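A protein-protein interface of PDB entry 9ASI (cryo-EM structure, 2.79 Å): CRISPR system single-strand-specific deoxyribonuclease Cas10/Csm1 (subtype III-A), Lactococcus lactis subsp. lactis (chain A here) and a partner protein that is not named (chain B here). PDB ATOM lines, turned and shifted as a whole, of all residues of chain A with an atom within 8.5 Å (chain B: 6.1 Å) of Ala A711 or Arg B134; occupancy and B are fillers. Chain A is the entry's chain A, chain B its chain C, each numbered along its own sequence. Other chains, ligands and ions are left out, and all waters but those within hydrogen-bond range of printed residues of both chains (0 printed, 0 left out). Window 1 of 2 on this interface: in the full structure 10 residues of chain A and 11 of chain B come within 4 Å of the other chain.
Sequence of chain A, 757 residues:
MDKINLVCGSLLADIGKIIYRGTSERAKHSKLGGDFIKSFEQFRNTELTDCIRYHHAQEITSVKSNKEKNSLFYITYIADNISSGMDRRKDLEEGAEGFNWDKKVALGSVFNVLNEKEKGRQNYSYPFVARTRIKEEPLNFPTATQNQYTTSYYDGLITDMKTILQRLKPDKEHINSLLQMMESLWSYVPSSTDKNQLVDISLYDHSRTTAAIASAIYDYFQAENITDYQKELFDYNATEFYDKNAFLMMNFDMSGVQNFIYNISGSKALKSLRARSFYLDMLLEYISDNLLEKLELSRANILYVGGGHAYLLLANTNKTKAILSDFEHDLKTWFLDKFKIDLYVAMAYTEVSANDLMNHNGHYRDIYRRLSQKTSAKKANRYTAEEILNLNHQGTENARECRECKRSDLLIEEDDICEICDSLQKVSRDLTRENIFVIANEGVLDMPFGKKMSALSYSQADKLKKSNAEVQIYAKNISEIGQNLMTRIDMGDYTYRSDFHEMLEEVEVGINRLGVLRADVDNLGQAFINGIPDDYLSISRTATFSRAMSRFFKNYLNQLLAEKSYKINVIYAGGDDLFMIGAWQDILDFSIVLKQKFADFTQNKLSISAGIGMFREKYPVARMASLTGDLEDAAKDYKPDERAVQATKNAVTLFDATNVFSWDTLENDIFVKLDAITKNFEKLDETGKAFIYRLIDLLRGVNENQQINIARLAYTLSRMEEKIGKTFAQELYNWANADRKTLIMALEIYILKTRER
Printed residues of chain B within 4 Å of Ile A710: Phe B26 and Gly B27. Of chain B, only Arg B134 (3.2 Å) comes within 4 Å of Ala A711. Of the printed residues of chain B, Tyr A715 touches Arg B134 and Glu B137. Of the printed residues of chain A, Phe B26 touches Gln A707 and Ile A710. Printed residues of chain A within 4 Å of Gly B27: Ile A710. Leu B130 touches none of the printed residues of chain A. No residue of chain A comes within 4 Å of Ala B133. Arg B134 touches just these residues of chain A: Ala A711 and Tyr A715. Of the printed residues of chain A, Glu B137 touches Tyr A715. The nearest residue of chain B that does not touch Ala A711 is Phe B26 (4.2 Å). The nearest residue of chain A that does not touch Arg B134 is Ala A714 (4.5 Å). The nearest printed residue of chain A that does not touch Phe B26 is Ala A711 (4.2 Å).
OH of Tyr A715 lies close to NH1 of Arg B134, at 2.3 Å.
Of the 16 printed residues of chain A, 4 touch a printed residue of chain B. Hydrophobic or aromatic side chains of chain A that line the printed part of chain B: Ile A710, Ala A711 and Tyr A715. Of the 14 printed residues of chain B, 4 touch a printed residue of chain A. Printed residues of chain B that touch a printed residue of chain A: Phe B26, Gly B27, Arg B134 and Glu B137. Hydrophobic or aromatic side chains of chain B that line the printed part of chain A: Phe B26. Among the printed residues, 6 pairs touch across the chains.
The guanidinium group of Arg B134 is in salt-bridge range of the side-chain carboxylate of Glu B137 (3.0 Å). The backbone carbonyl oxygen (O) of Arg B134 is in hydrogen-bond range of the side-chain hydroxyl (OG) of Ser B138, 3.0 Å away.
Gln A707 touches Phe B26 (O to CZ, 3.7 Å). Ile A710 touches Phe B26 (CG2 to CZ, 3.6 Å). Gly B27 touches Ile A710 (N to CD1, 3.4 Å). NH2 of Arg B134 touches CB of Ala A711 (3.2 Å). Glu B137 touches Tyr A715 (OE1 to CE1, 3.0 Å).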
ATOM      1  N   ARG A 694     -17.835  26.453 -31.901  1.00  0.00           N
ATOM      2  CA  ARG A 694     -18.295  26.272 -30.529  1.00  0.00           C
ATOM      3  C   ARG A 694     -19.579  27.055 -30.286  1.00  0.00           C
ATOM      4  O   ARG A 694     -20.587  26.503 -29.826  1.00  0.00           O
ATOM      5  CB  ARG A 694     -17.190  26.715 -29.571  1.00  0.00           C
ATOM      6  CG  ARG A 694     -17.421  26.430 -28.107  1.00  0.00           C
ATOM      7  CD  ARG A 694     -16.090  26.514 -27.379  1.00  0.00           C
ATOM      8  NE  ARG A 694     -15.547  27.866 -27.416  1.00  0.00           N
ATOM      9  CZ  ARG A 694     -15.209  28.568 -26.344  1.00  0.00           C
ATOM     10  NH1 ARG A 694     -15.295  28.056 -25.130  1.00  0.00           N
ATOM     11  NH2 ARG A 694     -14.765  29.813 -26.495  1.00  0.00           N
ATOM     12  N   LEU A 695     -19.565  28.342 -30.638  1.00  0.00           N
ATOM     13  CA  LEU A 695     -20.757  29.173 -30.501  1.00  0.00           C
ATOM     14  C   LEU A 695     -21.903  28.637 -31.348  1.00  0.00           C
ATOM     15  O   LEU A 695     -23.052  28.593 -30.892  1.00  0.00           O
ATOM     16  CB  LEU A 695     -20.436  30.615 -30.899  1.00  0.00           C
ATOM     17  CG  LEU A 695     -19.411  31.368 -30.054  1.00  0.00           C
ATOM     18  CD1 LEU A 695     -19.039  32.684 -30.718  1.00  0.00           C
ATOM     19  CD2 LEU A 695     -19.942  31.604 -28.652  1.00  0.00           C
ATOM     20  N   LEU A 698     -23.331  25.407 -29.891  1.00  0.00           N
ATOM     21  CA  LEU A 698     -23.964  25.605 -28.595  1.00  0.00           C
ATOM     22  C   LEU A 698     -25.133  26.580 -28.641  1.00  0.00           C
ATOM     23  O   LEU A 698     -25.844  26.716 -27.640  1.00  0.00           O
ATOM     24  CB  LEU A 698     -22.938  26.074 -27.560  1.00  0.00           C
ATOM     25  CG  LEU A 698     -22.215  24.927 -26.849  1.00  0.00           C
ATOM     26  CD1 LEU A 698     -23.241  24.070 -26.123  1.00  0.00           C
ATOM     27  CD2 LEU A 698     -21.369  24.081 -27.791  1.00  0.00           C
ATOM     28  N   GLN A 706     -28.499  25.537 -20.141  1.00  0.00           N
ATOM     29  CA  GLN A 706     -27.999  26.880 -20.393  1.00  0.00           C
ATOM     30  C   GLN A 706     -26.594  27.086 -19.855  1.00  0.00           C
ATOM     31  O   GLN A 706     -25.999  28.142 -20.103  1.00  0.00           O
ATOM     32  CB  GLN A 706     -28.931  27.915 -19.757  1.00  0.00           C
ATOM     33  CG  GLN A 706     -30.389  27.793 -20.161  1.00  0.00           C
ATOM     34  CD  GLN A 706     -30.657  28.340 -21.543  1.00  0.00           C
ATOM     35  OE1 GLN A 706     -30.072  29.343 -21.947  1.00  0.00           O
ATOM     36  NE2 GLN A 706     -31.561  27.694 -22.270  1.00  0.00           N
ATOM     37  N   GLN A 707     -26.060  26.100 -19.131  1.00  0.00           N
ATOM     38  CA  GLN A 707     -24.797  26.270 -18.425  1.00  0.00           C
ATOM     39  C   GLN A 707     -23.665  26.568 -19.394  1.00  0.00           C
ATOM     40  O   GLN A 707     -22.796  27.402 -19.114  1.00  0.00           O
ATOM     41  CB  GLN A 707     -24.482  25.005 -17.630  1.00  0.00           C
ATOM     42  CG  GLN A 707     -25.452  24.745 -16.507  1.00  0.00           C
ATOM     43  CD  GLN A 707     -26.713  24.070 -16.993  1.00  0.00           C
ATOM     44  OE1 GLN A 707     -26.735  23.515 -18.083  1.00  0.00           O
ATOM     45  NE2 GLN A 707     -27.782  24.159 -16.215  1.00  0.00           N
ATOM     46  N   ILE A 708     -23.656  25.889 -20.539  1.00  0.00           N
ATOM     47  CA  ILE A 708     -22.542  26.036 -21.461  1.00  0.00           C
ATOM     48  C   ILE A 708     -22.581  27.401 -22.136  1.00  0.00           C
ATOM     49  O   ILE A 708     -21.537  27.957 -22.481  1.00  0.00           O
ATOM     50  CB  ILE A 708     -22.529  24.886 -22.486  1.00  0.00           C
ATOM     51  CG1 ILE A 708     -22.444  23.527 -21.784  1.00  0.00           C
ATOM     52  CG2 ILE A 708     -21.318  25.005 -23.373  1.00  0.00           C
ATOM     53  CD1 ILE A 708     -23.785  22.883 -21.475  1.00  0.00           C
ATOM     54  N   ASN A 709     -23.772  27.976 -22.320  1.00  0.00           N
ATOM     55  CA  ASN A 709     -23.861  29.299 -22.934  1.00  0.00           C
ATOM     56  C   ASN A 709     -23.246  30.372 -22.040  1.00  0.00           C
ATOM     57  O   ASN A 709     -22.409  31.169 -22.486  1.00  0.00           O
ATOM     58  CB  ASN A 709     -25.321  29.626 -23.250  1.00  0.00           C
ATOM     59  CG  ASN A 709     -25.850  28.843 -24.437  1.00  0.00           C
ATOM     60  OD1 ASN A 709     -26.631  27.905 -24.279  1.00  0.00           O
ATOM     61  ND2 ASN A 709     -25.423  29.224 -25.634  1.00  0.00           N
ATOM     62  N   ILE A 710     -23.644  30.405 -20.765  1.00  0.00           N
ATOM     63  CA  ILE A 710     -23.040  31.352 -19.834  1.00  0.00           C
ATOM     64  C   ILE A 710     -21.566  31.022 -19.620  1.00  0.00           C
ATOM     65  O   ILE A 710     -20.750  31.920 -19.378  1.00  0.00           O
ATOM     66  CB  ILE A 710     -23.835  31.378 -18.512  1.00  0.00           C
ATOM     67  CG1 ILE A 710     -23.219  32.357 -17.510  1.00  0.00           C
ATOM     68  CG2 ILE A 710     -23.946  29.993 -17.911  1.00  0.00           C
ATOM     69  CD1 ILE A 710     -24.076  32.578 -16.280  1.00  0.00           C
ATOM     70  N   ALA A 711     -21.193  29.745 -19.733  1.00  0.00           N
ATOM     71  CA  ALA A 711     -19.783  29.376 -19.651  1.00  0.00           C
ATOM     72  C   ALA A 711     -18.981  29.969 -20.805  1.00  0.00           C
ATOM     73  O   ALA A 711     -17.871  30.474 -20.604  1.00  0.00           O
ATOM     74  CB  ALA A 711     -19.645  27.856 -19.629  1.00  0.00           C
ATOM     75  N   ARG A 712     -19.519  29.907 -22.025  1.00  0.00           N
ATOM     76  CA  ARG A 712     -18.844  30.526 -23.161  1.00  0.00           C
ATOM     77  C   ARG A 712     -18.798  32.038 -23.015  1.00  0.00           C
ATOM     78  O   ARG A 712     -17.828  32.673 -23.440  1.00  0.00           O
ATOM     79  CB  ARG A 712     -19.529  30.153 -24.477  1.00  0.00           C
ATOM     80  CG  ARG A 712     -19.636  28.663 -24.769  1.00  0.00           C
ATOM     81  CD  ARG A 712     -18.415  27.873 -24.320  1.00  0.00           C
ATOM     82  NE  ARG A 712     -18.638  26.438 -24.451  1.00  0.00           N
ATOM     83  CZ  ARG A 712     -17.741  25.501 -24.172  1.00  0.00           C
ATOM     84  NH1 ARG A 712     -16.535  25.810 -23.729  1.00  0.00           N
ATOM     85  NH2 ARG A 712     -18.066  24.223 -24.337  1.00  0.00           N
ATOM     86  N   LEU A 713     -19.842  32.629 -22.434  1.00  0.00           N
ATOM     87  CA  LEU A 713     -19.800  34.054 -22.122  1.00  0.00           C
ATOM     88  C   LEU A 713     -18.637  34.370 -21.187  1.00  0.00           C
ATOM     89  O   LEU A 713     -17.870  35.316 -21.417  1.00  0.00           O
ATOM     90  CB  LEU A 713     -21.128  34.483 -21.498  1.00  0.00           C
ATOM     91  CG  LEU A 713     -21.125  35.824 -20.770  1.00  0.00           C
ATOM     92  CD1 LEU A 713     -20.877  36.944 -21.754  1.00  0.00           C
ATOM     93  CD2 LEU A 713     -22.430  36.037 -20.022  1.00  0.00           C
ATOM     94  N   ALA A 714     -18.484  33.567 -20.132  1.00  0.00           N
ATOM     95  CA  ALA A 714     -17.385  33.766 -19.194  1.00  0.00           C
ATOM     96  C   ALA A 714     -16.036  33.577 -19.877  1.00  0.00           C
ATOM     97  O   ALA A 714     -15.082  34.303 -19.587  1.00  0.00           O
ATOM     98  CB  ALA A 714     -17.529  32.815 -18.008  1.00  0.00           C
ATOM     99  N   TYR A 715     -15.935  32.599 -20.780  1.00  0.00           N
ATOM    100  CA  TYR A 715     -14.688  32.374 -21.510  1.00  0.00           C
ATOM    101  C   TYR A 715     -14.350  33.553 -22.416  1.00  0.00           C
ATOM    102  O   TYR A 715     -13.182  33.948 -22.525  1.00  0.00           O
ATOM    103  CB  TYR A 715     -14.781  31.092 -22.334  1.00  0.00           C
ATOM    104  CG  TYR A 715     -14.809  29.822 -21.519  1.00  0.00           C
ATOM    105  CD1 TYR A 715     -14.565  29.840 -20.157  1.00  0.00           C
ATOM    106  CD2 TYR A 715     -15.076  28.602 -22.118  1.00  0.00           C
ATOM    107  CE1 TYR A 715     -14.589  28.679 -19.418  1.00  0.00           C
ATOM    108  CE2 TYR A 715     -15.102  27.436 -21.387  1.00  0.00           C
ATOM    109  CZ  TYR A 715     -14.858  27.479 -20.036  1.00  0.00           C
ATOM    110  OH  TYR A 715     -14.883  26.315 -19.301  1.00  0.00           O
ATOM    111  N   THR A 716     -15.353  34.104 -23.100  1.00  0.00           N
ATOM    112  CA  THR A 716     -15.125  35.274 -23.941  1.00  0.00           C
ATOM    113  C   THR A 716     -14.665  36.456 -23.101  1.00  0.00           C
ATOM    114  O   THR A 716     -13.789  37.222 -23.517  1.00  0.00           O
ATOM    115  CB  THR A 716     -16.398  35.625 -24.713  1.00  0.00           C
ATOM    116  OG1 THR A 716     -16.863  34.470 -25.422  1.00  0.00           O
ATOM    117  CG2 THR A 716     -16.126  36.741 -25.710  1.00  0.00           C
ATOM    118  N   LEU A 717     -15.250  36.618 -21.912  1.00  0.00           N
ATOM    119  CA  LEU A 717     -14.771  37.641 -20.986  1.00  0.00           C
ATOM    120  C   LEU A 717     -13.333  37.365 -20.561  1.00  0.00           C
ATOM    121  O   LEU A 717     -12.520  38.289 -20.442  1.00  0.00           O
ATOM    122  CB  LEU A 717     -15.684  37.707 -19.764  1.00  0.00           C
ATOM    123  CG  LEU A 717     -16.874  38.673 -19.780  1.00  0.00           C
ATOM    124  CD1 LEU A 717     -16.418  40.120 -19.763  1.00  0.00           C
ATOM    125  CD2 LEU A 717     -17.778  38.416 -20.966  1.00  0.00           C
ATOM    126  N   SER A 718     -13.008  36.092 -20.324  1.00  0.00           N
ATOM    127  CA  SER A 718     -11.679  35.709 -19.861  1.00  0.00           C
ATOM    128  C   SER A 718     -10.612  36.004 -20.906  1.00  0.00           C
ATOM    129  O   SER A 718      -9.498  36.414 -20.564  1.00  0.00           O
ATOM    130  CB  SER A 718     -11.669  34.224 -19.499  1.00  0.00           C
ATOM    131  OG  SER A 718     -10.358  33.765 -19.234  1.00  0.00           O
ATOM    132  N   PHE B  26     -24.105  30.987 -12.307  1.00  0.00           N
ATOM    133  CA  PHE B  26     -22.813  31.139 -11.650  1.00  0.00           C
ATOM    134  C   PHE B  26     -22.010  32.313 -12.194  1.00  0.00           C
ATOM    135  O   PHE B  26     -21.341  33.007 -11.424  1.00  0.00           O
ATOM    136  CB  PHE B  26     -21.979  29.858 -11.775  1.00  0.00           C
ATOM    137  CG  PHE B  26     -21.862  29.335 -13.177  1.00  0.00           C
ATOM    138  CD1 PHE B  26     -20.886  29.823 -14.028  1.00  0.00           C
ATOM    139  CD2 PHE B  26     -22.707  28.344 -13.637  1.00  0.00           C
ATOM    140  CE1 PHE B  26     -20.768  29.349 -15.311  1.00  0.00           C
ATOM    141  CE2 PHE B  26     -22.589  27.864 -14.925  1.00  0.00           C
ATOM    142  CZ  PHE B  26     -21.619  28.367 -15.761  1.00  0.00           C
ATOM    143  N   GLY B  27     -22.058  32.549 -13.505  1.00  0.00           N
ATOM    144  CA  GLY B  27     -21.250  33.606 -14.090  1.00  0.00           C
ATOM    145  C   GLY B  27     -21.706  34.994 -13.688  1.00  0.00           C
ATOM    146  O   GLY B  27     -20.882  35.877 -13.431  1.00  0.00           O
ATOM    147  N   TYR B  68     -11.307  18.961 -10.005  1.00  0.00           N
ATOM    148  CA  TYR B  68     -12.068  19.040 -11.247  1.00  0.00           C
ATOM    149  C   TYR B  68     -11.540  18.053 -12.280  1.00  0.00           C
ATOM    150  O   TYR B  68     -12.321  17.387 -12.969  1.00  0.00           O
ATOM    151  CB  TYR B  68     -12.023  20.466 -11.793  1.00  0.00           C
ATOM    152  CG  TYR B  68     -12.722  20.648 -13.121  1.00  0.00           C
ATOM    153  CD1 TYR B  68     -13.972  20.092 -13.354  1.00  0.00           C
ATOM    154  CD2 TYR B  68     -12.133  21.381 -14.139  1.00  0.00           C
ATOM    155  CE1 TYR B  68     -14.611  20.259 -14.567  1.00  0.00           C
ATOM    156  CE2 TYR B  68     -12.764  21.553 -15.354  1.00  0.00           C
ATOM    157  CZ  TYR B  68     -14.002  20.990 -15.563  1.00  0.00           C
ATOM    158  OH  TYR B  68     -14.633  21.161 -16.773  1.00  0.00           O
ATOM    159  N   PHE B 129     -20.730  19.740  -7.520  1.00  0.00           N
ATOM    160  CA  PHE B 129     -19.332  20.148  -7.567  1.00  0.00           C
ATOM    161  C   PHE B 129     -18.960  20.721  -8.926  1.00  0.00           C
ATOM    162  O   PHE B 129     -18.124  21.624  -9.000  1.00  0.00           O
ATOM    163  CB  PHE B 129     -18.404  18.987  -7.224  1.00  0.00           C
ATOM    164  CG  PHE B 129     -16.952  19.366  -7.251  1.00  0.00           C
ATOM    165  CD1 PHE B 129     -16.402  20.112  -6.223  1.00  0.00           C
ATOM    166  CD2 PHE B 129     -16.146  19.010  -8.317  1.00  0.00           C
ATOM    167  CE1 PHE B 129     -15.072  20.480  -6.249  1.00  0.00           C
ATOM    168  CE2 PHE B 129     -14.817  19.376  -8.347  1.00  0.00           C
ATOM    169  CZ  PHE B 129     -14.279  20.112  -7.311  1.00  0.00           C
ATOM    170  N   LEU B 130     -19.549  20.205 -10.007  1.00  0.00           N
ATOM    171  CA  LEU B 130     -19.321  20.818 -11.313  1.00  0.00           C
ATOM    172  C   LEU B 130     -19.803  22.262 -11.334  1.00  0.00           C
ATOM    173  O   LEU B 130     -19.116  23.143 -11.861  1.00  0.00           O
ATOM    174  CB  LEU B 130     -20.002  20.004 -12.414  1.00  0.00           C
ATOM    175  CG  LEU B 130     -19.188  18.908 -13.105  1.00  0.00           C
ATOM    176  CD1 LEU B 130     -18.039  19.543 -13.867  1.00  0.00           C
ATOM    177  CD2 LEU B 130     -18.660  17.876 -12.128  1.00  0.00           C
ATOM    178  N   LEU B 131     -20.977  22.524 -10.758  1.00  0.00           N
ATOM    179  CA  LEU B 131     -21.473  23.893 -10.674  1.00  0.00           C
ATOM    180  C   LEU B 131     -20.558  24.764  -9.822  1.00  0.00           C
ATOM    181  O   LEU B 131     -20.278  25.916 -10.174  1.00  0.00           O
ATOM    182  CB  LEU B 131     -22.897  23.894 -10.118  1.00  0.00           C
ATOM    183  CG  LEU B 131     -23.463  25.211  -9.592  1.00  0.00           C
ATOM    184  CD1 LEU B 131     -23.529  26.257 -10.688  1.00  0.00           C
ATOM    185  CD2 LEU B 131     -24.835  24.971  -8.995  1.00  0.00           C
ATOM    186  N   PHE B 132     -20.083  24.231  -8.694  1.00  0.00           N
ATOM    187  CA  PHE B 132     -19.169  24.988  -7.841  1.00  0.00           C
ATOM    188  C   PHE B 132     -17.875  25.328  -8.575  1.00  0.00           C
ATOM    189  O   PHE B 132     -17.384  26.463  -8.501  1.00  0.00           O
ATOM    190  CB  PHE B 132     -18.876  24.189  -6.572  1.00  0.00           C
ATOM    191  CG  PHE B 132     -17.632  24.621  -5.853  1.00  0.00           C
ATOM    192  CD1 PHE B 132     -17.528  25.891  -5.318  1.00  0.00           C
ATOM    193  CD2 PHE B 132     -16.562  23.754  -5.718  1.00  0.00           C
ATOM    194  CE1 PHE B 132     -16.386  26.284  -4.655  1.00  0.00           C
ATOM    195  CE2 PHE B 132     -15.416  24.146  -5.061  1.00  0.00           C
ATOM    196  CZ  PHE B 132     -15.327  25.414  -4.533  1.00  0.00           C
ATOM    197  N   ALA B 133     -17.308  24.351  -9.288  1.00  0.00           N
ATOM    198  CA  ALA B 133     -16.083  24.585 -10.040  1.00  0.00           C
ATOM    199  C   ALA B 133     -16.310  25.586 -11.164  1.00  0.00           C
ATOM    200  O   ALA B 133     -15.445  26.423 -11.438  1.00  0.00           O
ATOM    201  CB  ALA B 133     -15.546  23.267 -10.591  1.00  0.00           C
ATOM    202  N   ARG B 134     -17.465  25.507 -11.832  1.00  0.00           N
ATOM    203  CA  ARG B 134     -17.799  26.490 -12.854  1.00  0.00           C
ATOM    204  C   ARG B 134     -17.879  27.887 -12.258  1.00  0.00           C
ATOM    205  O   ARG B 134     -17.410  28.858 -12.860  1.00  0.00           O
ATOM    206  CB  ARG B 134     -19.123  26.123 -13.523  1.00  0.00           C
ATOM    207  CG  ARG B 134     -19.042  25.010 -14.554  1.00  0.00           C
ATOM    208  CD  ARG B 134     -17.953  25.259 -15.580  1.00  0.00           C
ATOM    209  NE  ARG B 134     -17.918  26.645 -16.033  1.00  0.00           N
ATOM    210  CZ  ARG B 134     -17.324  27.051 -17.145  1.00  0.00           C
ATOM    211  NH1 ARG B 134     -16.740  26.197 -17.968  1.00  0.00           N
ATOM    212  NH2 ARG B 134     -17.315  28.349 -17.439  1.00  0.00           N
ATOM    213  N   TYR B 135     -18.475  28.003 -11.068  1.00  0.00           N
ATOM    214  CA  TYR B 135     -18.570  29.294 -10.398  1.00  0.00           C
ATOM    215  C   TYR B 135     -17.186  29.854 -10.085  1.00  0.00           C
ATOM    216  O   TYR B 135     -16.906  31.028 -10.351  1.00  0.00           O
ATOM    217  CB  TYR B 135     -19.412  29.145  -9.127  1.00  0.00           C
ATOM    218  CG  TYR B 135     -19.224  30.229  -8.087  1.00  0.00           C
ATOM    219  CD1 TYR B 135     -19.338  31.574  -8.420  1.00  0.00           C
ATOM    220  CD2 TYR B 135     -18.946  29.902  -6.766  1.00  0.00           C
ATOM    221  CE1 TYR B 135     -19.168  32.560  -7.467  1.00  0.00           C
ATOM    222  CE2 TYR B 135     -18.777  30.882  -5.809  1.00  0.00           C
ATOM    223  CZ  TYR B 135     -18.889  32.207  -6.164  1.00  0.00           C
ATOM    224  OH  TYR B 135     -18.720  33.182  -5.209  1.00  0.00           O
ATOM    225  N   VAL B 136     -16.298  29.021  -9.534  1.00  0.00           N
ATOM    226  CA  VAL B 136     -14.953  29.490  -9.195  1.00  0.00           C
ATOM    227  C   VAL B 136     -14.175  29.874 -10.450  1.00  0.00           C
ATOM    228  O   VAL B 136     -13.465  30.890 -10.478  1.00  0.00           O
ATOM    229  CB  VAL B 136     -14.201  28.426  -8.377  1.00  0.00           C
ATOM    230  CG1 VAL B 136     -12.812  28.926  -8.011  1.00  0.00           C
ATOM    231  CG2 VAL B 136     -14.980  28.076  -7.135  1.00  0.00           C
ATOM    232  N   GLU B 137     -14.274  29.054 -11.499  1.00  0.00           N
ATOM    233  CA  GLU B 137     -13.583  29.348 -12.747  1.00  0.00           C
ATOM    234  C   GLU B 137     -14.078  30.653 -13.356  1.00  0.00           C
ATOM    235  O   GLU B 137     -13.278  31.465 -13.833  1.00  0.00           O
ATOM    236  CB  GLU B 137     -13.770  28.185 -13.720  1.00  0.00           C
ATOM    237  CG  GLU B 137     -12.838  28.206 -14.914  1.00  0.00           C
ATOM    238  CD  GLU B 137     -13.401  29.018 -16.055  1.00  0.00           C
ATOM    239  OE1 GLU B 137     -14.551  28.746 -16.454  1.00  0.00           O
ATOM    240  OE2 GLU B 137     -12.701  29.929 -16.546  1.00  0.00           O
ATOM    241  N   SER B 138     -15.395  30.874 -13.345  1.00  0.00           N
ATOM    242  CA  SER B 138     -15.942  32.140 -13.820  1.00  0.00           C
ATOM    243  C   SER B 138     -15.466  33.300 -12.958  1.00  0.00           C
ATOM    244  O   SER B 138     -15.228  34.401 -13.463  1.00  0.00           O
ATOM    245  CB  SER B 138     -17.467  32.074 -13.832  1.00  0.00           C
ATOM    246  OG  SER B 138     -17.964  31.824 -12.530  1.00  0.00           O
ATOM    247  N   LEU B 139     -15.325  33.069 -11.653  1.00  0.00           N
ATOM    248  CA  LEU B 139     -14.825  34.104 -10.755  1.00  0.00           C
ATOM    249  C   LEU B 139     -13.415  34.537 -11.142  1.00  0.00           C
ATOM    250  O   LEU B 139     -13.113  35.734 -11.210  1.00  0.00           O
ATOM    251  CB  LEU B 139     -14.852  33.583  -9.323  1.00  0.00           C
ATOM    252  CG  LEU B 139     -14.906  34.579  -8.176  1.00  0.00           C
ATOM    253  CD1 LEU B 139     -16.076  35.518  -8.336  1.00  0.00           C
ATOM    254  CD2 LEU B 139     -15.042  33.795  -6.909  1.00  0.00           C
